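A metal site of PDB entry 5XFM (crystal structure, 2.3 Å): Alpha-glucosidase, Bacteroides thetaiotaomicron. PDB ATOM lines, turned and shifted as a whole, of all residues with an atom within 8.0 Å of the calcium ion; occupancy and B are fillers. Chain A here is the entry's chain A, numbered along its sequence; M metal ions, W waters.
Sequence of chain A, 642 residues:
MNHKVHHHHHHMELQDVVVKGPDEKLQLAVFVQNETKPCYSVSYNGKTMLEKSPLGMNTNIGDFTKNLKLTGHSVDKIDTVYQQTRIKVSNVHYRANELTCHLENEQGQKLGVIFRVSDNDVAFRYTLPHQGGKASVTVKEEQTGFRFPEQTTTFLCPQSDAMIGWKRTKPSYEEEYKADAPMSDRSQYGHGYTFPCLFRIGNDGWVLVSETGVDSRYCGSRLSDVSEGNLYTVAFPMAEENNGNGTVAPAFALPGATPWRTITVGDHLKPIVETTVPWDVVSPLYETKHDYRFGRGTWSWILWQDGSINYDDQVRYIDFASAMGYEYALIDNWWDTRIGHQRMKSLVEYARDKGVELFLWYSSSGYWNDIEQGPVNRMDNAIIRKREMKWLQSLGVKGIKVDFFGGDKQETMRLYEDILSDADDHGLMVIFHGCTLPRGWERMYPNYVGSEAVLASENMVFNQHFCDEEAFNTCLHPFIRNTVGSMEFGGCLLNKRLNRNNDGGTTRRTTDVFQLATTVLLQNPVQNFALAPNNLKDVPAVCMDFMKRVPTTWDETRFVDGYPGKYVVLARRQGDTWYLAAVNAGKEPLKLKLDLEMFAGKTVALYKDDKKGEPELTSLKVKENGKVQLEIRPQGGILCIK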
ATOM      1  N   TRP A 166      -2.851  -0.098  -4.708  1.00  0.00           N
ATOM      2  CA  TRP A 166      -4.073  -0.578  -5.343  1.00  0.00           C
ATOM      3  C   TRP A 166      -4.600   0.367  -6.420  1.00  0.00           C
ATOM      4  O   TRP A 166      -4.947   1.515  -6.134  1.00  0.00           O
ATOM      5  CB  TRP A 166      -5.155  -0.829  -4.286  1.00  0.00           C
ATOM      6  CG  TRP A 166      -6.464  -1.269  -4.846  1.00  0.00           C
ATOM      7  CD1 TRP A 166      -7.635  -0.570  -4.864  1.00  0.00           C
ATOM      8  CD2 TRP A 166      -6.756  -2.543  -5.464  1.00  0.00           C
ATOM      9  NE1 TRP A 166      -8.637  -1.317  -5.458  1.00  0.00           N
ATOM     10  CE2 TRP A 166      -8.115  -2.526  -5.830  1.00  0.00           C
ATOM     11  CE3 TRP A 166      -5.988  -3.685  -5.731  1.00  0.00           C
ATOM     12  CZ2 TRP A 166      -8.731  -3.618  -6.458  1.00  0.00           C
ATOM     13  CZ3 TRP A 166      -6.613  -4.766  -6.358  1.00  0.00           C
ATOM     14  CH2 TRP A 166      -7.966  -4.719  -6.716  1.00  0.00           C
ATOM     15  N   THR A 169      -3.585   4.158  -6.806  1.00  0.00           N
ATOM     16  CA  THR A 169      -4.259   5.161  -5.980  1.00  0.00           C
ATOM     17  C   THR A 169      -3.401   5.876  -4.933  1.00  0.00           C
ATOM     18  O   THR A 169      -3.887   6.780  -4.248  1.00  0.00           O
ATOM     19  CB  THR A 169      -5.455   4.559  -5.244  1.00  0.00           C
ATOM     20  OG1 THR A 169      -5.043   3.361  -4.575  1.00  0.00           O
ATOM     21  CG2 THR A 169      -6.563   4.215  -6.213  1.00  0.00           C
ATOM     22  N   SER A 172      -1.927   7.827  -0.339  1.00  0.00           N
ATOM     23  CA  SER A 172      -3.212   7.763   0.342  1.00  0.00           C
ATOM     24  C   SER A 172      -3.049   7.827   1.862  1.00  0.00           C
ATOM     25  O   SER A 172      -3.963   7.466   2.605  1.00  0.00           O
ATOM     26  CB  SER A 172      -3.976   6.495  -0.060  1.00  0.00           C
ATOM     27  OG  SER A 172      -3.134   5.340   0.021  1.00  0.00           O
ATOM     28  N   GLU A 174      -1.328   6.085   3.900  1.00  0.00           N
ATOM     29  CA  GLU A 174      -1.503   4.761   4.488  1.00  0.00           C
ATOM     30  C   GLU A 174      -0.162   4.050   4.652  1.00  0.00           C
ATOM     31  O   GLU A 174       0.069   3.001   4.070  1.00  0.00           O
ATOM     32  CB  GLU A 174      -2.471   3.931   3.621  1.00  0.00           C
ATOM     33  CG  GLU A 174      -3.939   4.210   3.936  1.00  0.00           C
ATOM     34  CD  GLU A 174      -4.901   3.753   2.834  1.00  0.00           C
ATOM     35  OE1 GLU A 174      -4.448   3.402   1.734  1.00  0.00           O
ATOM     36  OE2 GLU A 174      -6.116   3.732   3.088  1.00  0.00           O
ATOM     37  N   TRP A 301     -19.016  -4.452   4.658  1.00  0.00           N
ATOM     38  CA  TRP A 301     -17.834  -4.728   3.851  1.00  0.00           C
ATOM     39  C   TRP A 301     -16.562  -5.025   4.652  1.00  0.00           C
ATOM     40  O   TRP A 301     -15.700  -5.738   4.169  1.00  0.00           O
ATOM     41  CB  TRP A 301     -17.560  -3.561   2.894  1.00  0.00           C
ATOM     42  CG  TRP A 301     -16.336  -3.783   2.052  1.00  0.00           C
ATOM     43  CD1 TRP A 301     -16.269  -4.388   0.837  1.00  0.00           C
ATOM     44  CD2 TRP A 301     -14.991  -3.423   2.393  1.00  0.00           C
ATOM     45  NE1 TRP A 301     -14.963  -4.425   0.383  1.00  0.00           N
ATOM     46  CE2 TRP A 301     -14.164  -3.832   1.325  1.00  0.00           C
ATOM     47  CE3 TRP A 301     -14.404  -2.787   3.493  1.00  0.00           C
ATOM     48  CZ2 TRP A 301     -12.783  -3.627   1.338  1.00  0.00           C
ATOM     49  CZ3 TRP A 301     -13.041  -2.586   3.494  1.00  0.00           C
ATOM     50  CH2 TRP A 301     -12.237  -3.003   2.421  1.00  0.00           C
ATOM     51  N   TRP A 361     -21.281   4.787  -0.369  1.00  0.00           N
ATOM     52  CA  TRP A 361     -19.905   4.857  -0.889  1.00  0.00           C
ATOM     53  C   TRP A 361     -19.853   5.409  -2.304  1.00  0.00           C
ATOM     54  O   TRP A 361     -20.627   5.004  -3.174  1.00  0.00           O
ATOM     55  CB  TRP A 361     -19.264   3.466  -0.868  1.00  0.00           C
ATOM     56  CG  TRP A 361     -17.782   3.427  -1.155  1.00  0.00           C
ATOM     57  CD1 TRP A 361     -16.763   3.395  -0.235  1.00  0.00           C
ATOM     58  CD2 TRP A 361     -17.137   3.380  -2.447  1.00  0.00           C
ATOM     59  NE1 TRP A 361     -15.540   3.353  -0.870  1.00  0.00           N
ATOM     60  CE2 TRP A 361     -15.745   3.344  -2.227  1.00  0.00           C
ATOM     61  CE3 TRP A 361     -17.614   3.382  -3.764  1.00  0.00           C
ATOM     62  CZ2 TRP A 361     -14.820   3.303  -3.273  1.00  0.00           C
ATOM     63  CZ3 TRP A 361     -16.694   3.344  -4.796  1.00  0.00           C
ATOM     64  CH2 TRP A 361     -15.315   3.313  -4.543  1.00  0.00           C
ATOM     65  N   LYS A 401     -19.557   8.381   1.715  1.00  0.00           N
ATOM     66  CA  LYS A 401     -18.162   8.026   1.921  1.00  0.00           C
ATOM     67  C   LYS A 401     -17.429   8.098   0.582  1.00  0.00           C
ATOM     68  O   LYS A 401     -17.702   7.292  -0.314  1.00  0.00           O
ATOM     69  CB  LYS A 401     -18.044   6.646   2.546  1.00  0.00           C
ATOM     70  CG  LYS A 401     -16.616   6.111   2.681  1.00  0.00           C
ATOM     71  CD  LYS A 401     -16.597   4.716   3.239  1.00  0.00           C
ATOM     72  CE  LYS A 401     -15.194   4.142   3.246  1.00  0.00           C
ATOM     73  NZ  LYS A 401     -15.143   2.758   3.764  1.00  0.00           N
ATOM     74  N   ASP A 403     -13.974   8.077  -1.781  1.00  0.00           N
ATOM     75  CA  ASP A 403     -12.700   7.360  -1.699  1.00  0.00           C
ATOM     76  C   ASP A 403     -11.738   7.665  -2.860  1.00  0.00           C
ATOM     77  O   ASP A 403     -12.128   8.275  -3.855  1.00  0.00           O
ATOM     78  CB  ASP A 403     -12.976   5.857  -1.663  1.00  0.00           C
ATOM     79  CG  ASP A 403     -11.979   5.100  -0.795  1.00  0.00           C
ATOM     80  OD1 ASP A 403     -10.817   5.548  -0.707  1.00  0.00           O
ATOM     81  OD2 ASP A 403     -12.372   4.066  -0.209  1.00  0.00           O
ATOM     82  N   PHE A 404     -10.488   7.266  -2.687  1.00  0.00           N
ATOM     83  CA  PHE A 404      -9.474   7.224  -3.758  1.00  0.00           C
ATOM     84  C   PHE A 404      -9.147   8.567  -4.426  1.00  0.00           C
ATOM     85  O   PHE A 404      -9.212   8.694  -5.648  1.00  0.00           O
ATOM     86  CB  PHE A 404      -9.885   6.239  -4.851  1.00  0.00           C
ATOM     87  CG  PHE A 404     -10.034   4.815  -4.370  1.00  0.00           C
ATOM     88  CD1 PHE A 404      -9.019   4.206  -3.654  1.00  0.00           C
ATOM     89  CD2 PHE A 404     -11.184   4.103  -4.642  1.00  0.00           C
ATOM     90  CE1 PHE A 404      -9.146   2.903  -3.220  1.00  0.00           C
ATOM     91  CE2 PHE A 404     -11.329   2.802  -4.191  1.00  0.00           C
ATOM     92  CZ  PHE A 404     -10.305   2.202  -3.491  1.00  0.00           C
ATOM     93  N   PHE A 432     -14.201  11.084   4.164  1.00  0.00           N
ATOM     94  CA  PHE A 432     -13.202  10.847   3.128  1.00  0.00           C
ATOM     95  C   PHE A 432     -12.371   9.598   3.408  1.00  0.00           C
ATOM     96  O   PHE A 432     -12.012   9.329   4.554  1.00  0.00           O
ATOM     97  CB  PHE A 432     -12.258  12.035   2.969  1.00  0.00           C
ATOM     98  CG  PHE A 432     -12.923  13.250   2.405  1.00  0.00           C
ATOM     99  CD1 PHE A 432     -13.702  13.162   1.259  1.00  0.00           C
ATOM    100  CD2 PHE A 432     -12.750  14.481   3.006  1.00  0.00           C
ATOM    101  CE1 PHE A 432     -14.303  14.286   0.746  1.00  0.00           C
ATOM    102  CE2 PHE A 432     -13.360  15.607   2.489  1.00  0.00           C
ATOM    103  CZ  PHE A 432     -14.134  15.512   1.355  1.00  0.00           C
ATOM    104  N   HIS A 433     -12.084   8.856   2.348  1.00  0.00           N
ATOM    105  CA  HIS A 433     -11.179   7.706   2.417  1.00  0.00           C
ATOM    106  C   HIS A 433     -10.189   7.780   1.270  1.00  0.00           C
ATOM    107  O   HIS A 433     -10.395   8.519   0.302  1.00  0.00           O
ATOM    108  CB  HIS A 433     -11.950   6.397   2.376  1.00  0.00           C
ATOM    109  CG  HIS A 433     -12.310   5.857   3.732  1.00  0.00           C
ATOM    110  ND1 HIS A 433     -11.879   4.630   4.176  1.00  0.00           N
ATOM    111  CD2 HIS A 433     -13.053   6.375   4.730  1.00  0.00           C
ATOM    112  CE1 HIS A 433     -12.332   4.421   5.395  1.00  0.00           C
ATOM    113  NE2 HIS A 433     -13.053   5.472   5.754  1.00  0.00           N
ATOM    114  N   GLY A 434      -9.096   7.020   1.376  1.00  0.00           N
ATOM    115  CA  GLY A 434      -8.063   6.987   0.347  1.00  0.00           C
ATOM    116  C   GLY A 434      -7.586   8.399   0.118  1.00  0.00           C
ATOM    117  O   GLY A 434      -7.456   8.836  -1.031  1.00  0.00           O
ATOM    118  N   CYS A 435      -7.307   9.087   1.210  1.00  0.00           N
ATOM    119  CA  CYS A 435      -7.300  10.548   1.223  1.00  0.00           C
ATOM    120  C   CYS A 435      -6.136  11.138   1.990  1.00  0.00           C
ATOM    121  O   CYS A 435      -5.332  10.418   2.596  1.00  0.00           O
ATOM    122  CB  CYS A 435      -8.611  11.055   1.828  1.00  0.00           C
ATOM    123  SG  CYS A 435      -8.869  10.521   3.558  1.00  0.00           S
ATOM    124  N   GLU A 452      -9.977   9.047   6.488  1.00  0.00           N
ATOM    125  CA  GLU A 452      -9.194   7.846   6.728  1.00  0.00           C
ATOM    126  C   GLU A 452      -7.748   8.298   7.026  1.00  0.00           C
ATOM    127  O   GLU A 452      -7.395   8.488   8.186  1.00  0.00           O
ATOM    128  CB  GLU A 452      -9.260   6.887   5.529  1.00  0.00           C
ATOM    129  CG  GLU A 452      -8.676   5.490   5.760  1.00  0.00           C
ATOM    130  CD  GLU A 452      -8.726   4.630   4.511  1.00  0.00           C
ATOM    131  OE1 GLU A 452      -8.658   5.204   3.390  1.00  0.00           O
ATOM    132  OE2 GLU A 452      -8.831   3.383   4.614  1.00  0.00           O
ATOM    133  N   ALA A 453      -6.953   8.505   5.982  1.00  0.00           N
ATOM    134  CA  ALA A 453      -5.570   8.993   6.107  1.00  0.00           C
ATOM    135  C   ALA A 453      -4.790   8.242   7.174  1.00  0.00           C
ATOM    136  O   ALA A 453      -4.033   8.834   7.947  1.00  0.00           O
ATOM    137  CB  ALA A 453      -5.564  10.489   6.412  1.00  0.00           C
ATOM    138  N   VAL A 454      -4.948   6.921   7.190  1.00  0.00           N
ATOM    139  CA  VAL A 454      -4.285   6.058   8.162  1.00  0.00           C
ATOM    140  C   VAL A 454      -4.433   4.626   7.680  1.00  0.00           C
ATOM    141  O   VAL A 454      -5.324   4.323   6.863  1.00  0.00           O
ATOM    142  CB  VAL A 454      -4.898   6.211   9.585  1.00  0.00           C
ATOM    143  CG1 VAL A 454      -6.310   5.628   9.621  1.00  0.00           C
ATOM    144  CG2 VAL A 454      -4.044   5.537  10.635  1.00  0.00           C
ATOM    145  N   LEU A 455      -3.569   3.752   8.168  1.00  0.00           N
ATOM    146  CA  LEU A 455      -3.732   2.328   7.967  1.00  0.00           C
ATOM    147  C   LEU A 455      -4.904   1.873   8.827  1.00  0.00           C
ATOM    148  O   LEU A 455      -4.754   1.617  10.026  1.00  0.00           O
ATOM    149  CB  LEU A 455      -2.430   1.591   8.313  1.00  0.00           C
ATOM    150  CG  LEU A 455      -1.401   1.727   7.198  1.00  0.00           C
ATOM    151  CD1 LEU A 455      -0.014   1.363   7.654  1.00  0.00           C
ATOM    152  CD2 LEU A 455      -1.814   0.849   6.023  1.00  0.00           C
ATOM    153  N   ALA A 456      -6.071   1.798   8.212  1.00  0.00           N
ATOM    154  CA  ALA A 456      -7.293   1.473   8.935  1.00  0.00           C
ATOM    155  C   ALA A 456      -7.428  -0.022   9.203  1.00  0.00           C
ATOM    156  O   ALA A 456      -6.582  -0.820   8.804  1.00  0.00           O
ATOM    157  CB  ALA A 456      -8.521   1.986   8.180  1.00  0.00           C
ATOM    158  N   GLU A 458      -9.149  -2.213   7.952  1.00  0.00           N
ATOM    159  CA  GLU A 458      -9.210  -3.023   6.738  1.00  0.00           C
ATOM    160  C   GLU A 458      -7.901  -3.795   6.537  1.00  0.00           C
ATOM    161  O   GLU A 458      -7.900  -4.938   6.089  1.00  0.00           O
ATOM    162  CB  GLU A 458      -9.518  -2.160   5.509  1.00  0.00           C
ATOM    163  CG  GLU A 458      -8.371  -1.254   5.048  1.00  0.00           C
ATOM    164  CD  GLU A 458      -8.682  -0.469   3.774  1.00  0.00           C
ATOM    165  OE1 GLU A 458      -9.615  -0.849   3.030  1.00  0.00           O
ATOM    166  OE2 GLU A 458      -7.961   0.528   3.502  1.00  0.00           O
ATOM    167  N   ASN A 459      -6.784  -3.166   6.911  1.00  0.00           N
ATOM    168  CA  ASN A 459      -5.487  -3.787   6.711  1.00  0.00           C
ATOM    169  C   ASN A 459      -5.348  -5.023   7.600  1.00  0.00           C
ATOM    170  O   ASN A 459      -4.741  -6.014   7.208  1.00  0.00           O
ATOM    171  CB  ASN A 459      -4.366  -2.774   6.970  1.00  0.00           C
ATOM    172  CG  ASN A 459      -4.385  -1.628   5.971  1.00  0.00           C
ATOM    173  OD1 ASN A 459      -4.713  -0.491   6.314  1.00  0.00           O
ATOM    174  ND2 ASN A 459      -4.035  -1.924   4.726  1.00  0.00           N
ATOM    175  N   PHE A 462      -6.788  -7.618   5.778  1.00  0.00           N
ATOM    176  CA  PHE A 462      -5.988  -7.982   4.617  1.00  0.00           C
ATOM    177  C   PHE A 462      -4.751  -8.807   4.977  1.00  0.00           C
ATOM    178  O   PHE A 462      -4.392  -9.731   4.258  1.00  0.00           O
ATOM    179  CB  PHE A 462      -5.535  -6.737   3.850  1.00  0.00           C
ATOM    180  CG  PHE A 462      -6.661  -5.904   3.312  1.00  0.00           C
ATOM    181  CD1 PHE A 462      -7.879  -6.484   2.999  1.00  0.00           C
ATOM    182  CD2 PHE A 462      -6.499  -4.547   3.099  1.00  0.00           C
ATOM    183  CE1 PHE A 462      -8.913  -5.719   2.490  1.00  0.00           C
ATOM    184  CE2 PHE A 462      -7.533  -3.774   2.595  1.00  0.00           C
ATOM    185  CZ  PHE A 462      -8.737  -4.363   2.297  1.00  0.00           C
HETATM  186 CA    CA M   1      -8.349   2.790   2.317  1.00  0.00          CA
HETATM  187  O   HOH W   1     -10.750   2.758   2.124  1.00  0.00           O
HETATM  188  O   HOH W   2      -6.809   1.523   0.803  1.00  0.00           O
HETATM  189  O   HOH W   3      -8.478   3.860   0.225  1.00  0.00           O
HETATM  190  O   HOH W   4      -8.825   0.442   0.779  1.00  0.00           O
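Three residues have an atom within 4 Å of the calcium ion: Glu 174, Glu 452 and Glu 458. The nearest printed residue that does not touch the calcium ion is His 433 (4.4 Å).
Water W3 bridges the side-chain carboxylate of Asp 403 (3.0 Å) and the backbone NH of Gly 434 (3.4 Å). Water W1 lies within hydrogen-bond range of a ring nitrogen (ND1) of His 433 (3.0 Å) and the side-chain carboxylate (OD2) of Asp 403 (3.1 Å).
Water W3 is bound to the calcium ion (2.4 Å). The calcium ion is bound by water W1 (2.4 Å). The side-chain carboxylate (OE2) of Glu 452 binds the calcium ion. The calcium ion is bound by water W2. OE2 of Glu 174 is bound to the calcium ion, 2.5 Å away. OE2 of Glu 458 binds the calcium ion (2.6 Å). The side-chain carboxylate (OE1) of Glu 452 binds the calcium ion (2.7 Å). Water W4 is bound to the calcium ion, 2.8 Å away.
The side-chain carboxylate (OE1) of Glu 174 sits at hydrogen-bond distance from the side-chain hydroxyl (OG) of Ser 172 (2.9 Å). The backbone NH (N) of Glu 452 is in hydrogen-bond range of the side-chain sulfur (SG) of Cys 435, at 3.5 Å. O of Phe 432 sits at hydrogen-bond distance from N of Glu 452 (2.8 Å). A ring nitrogen (ND1) of His 433 lies close to the side-chain carboxylate (OE2) of Glu 452. N of Gly 434 sits close to OE1 of Glu 452.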
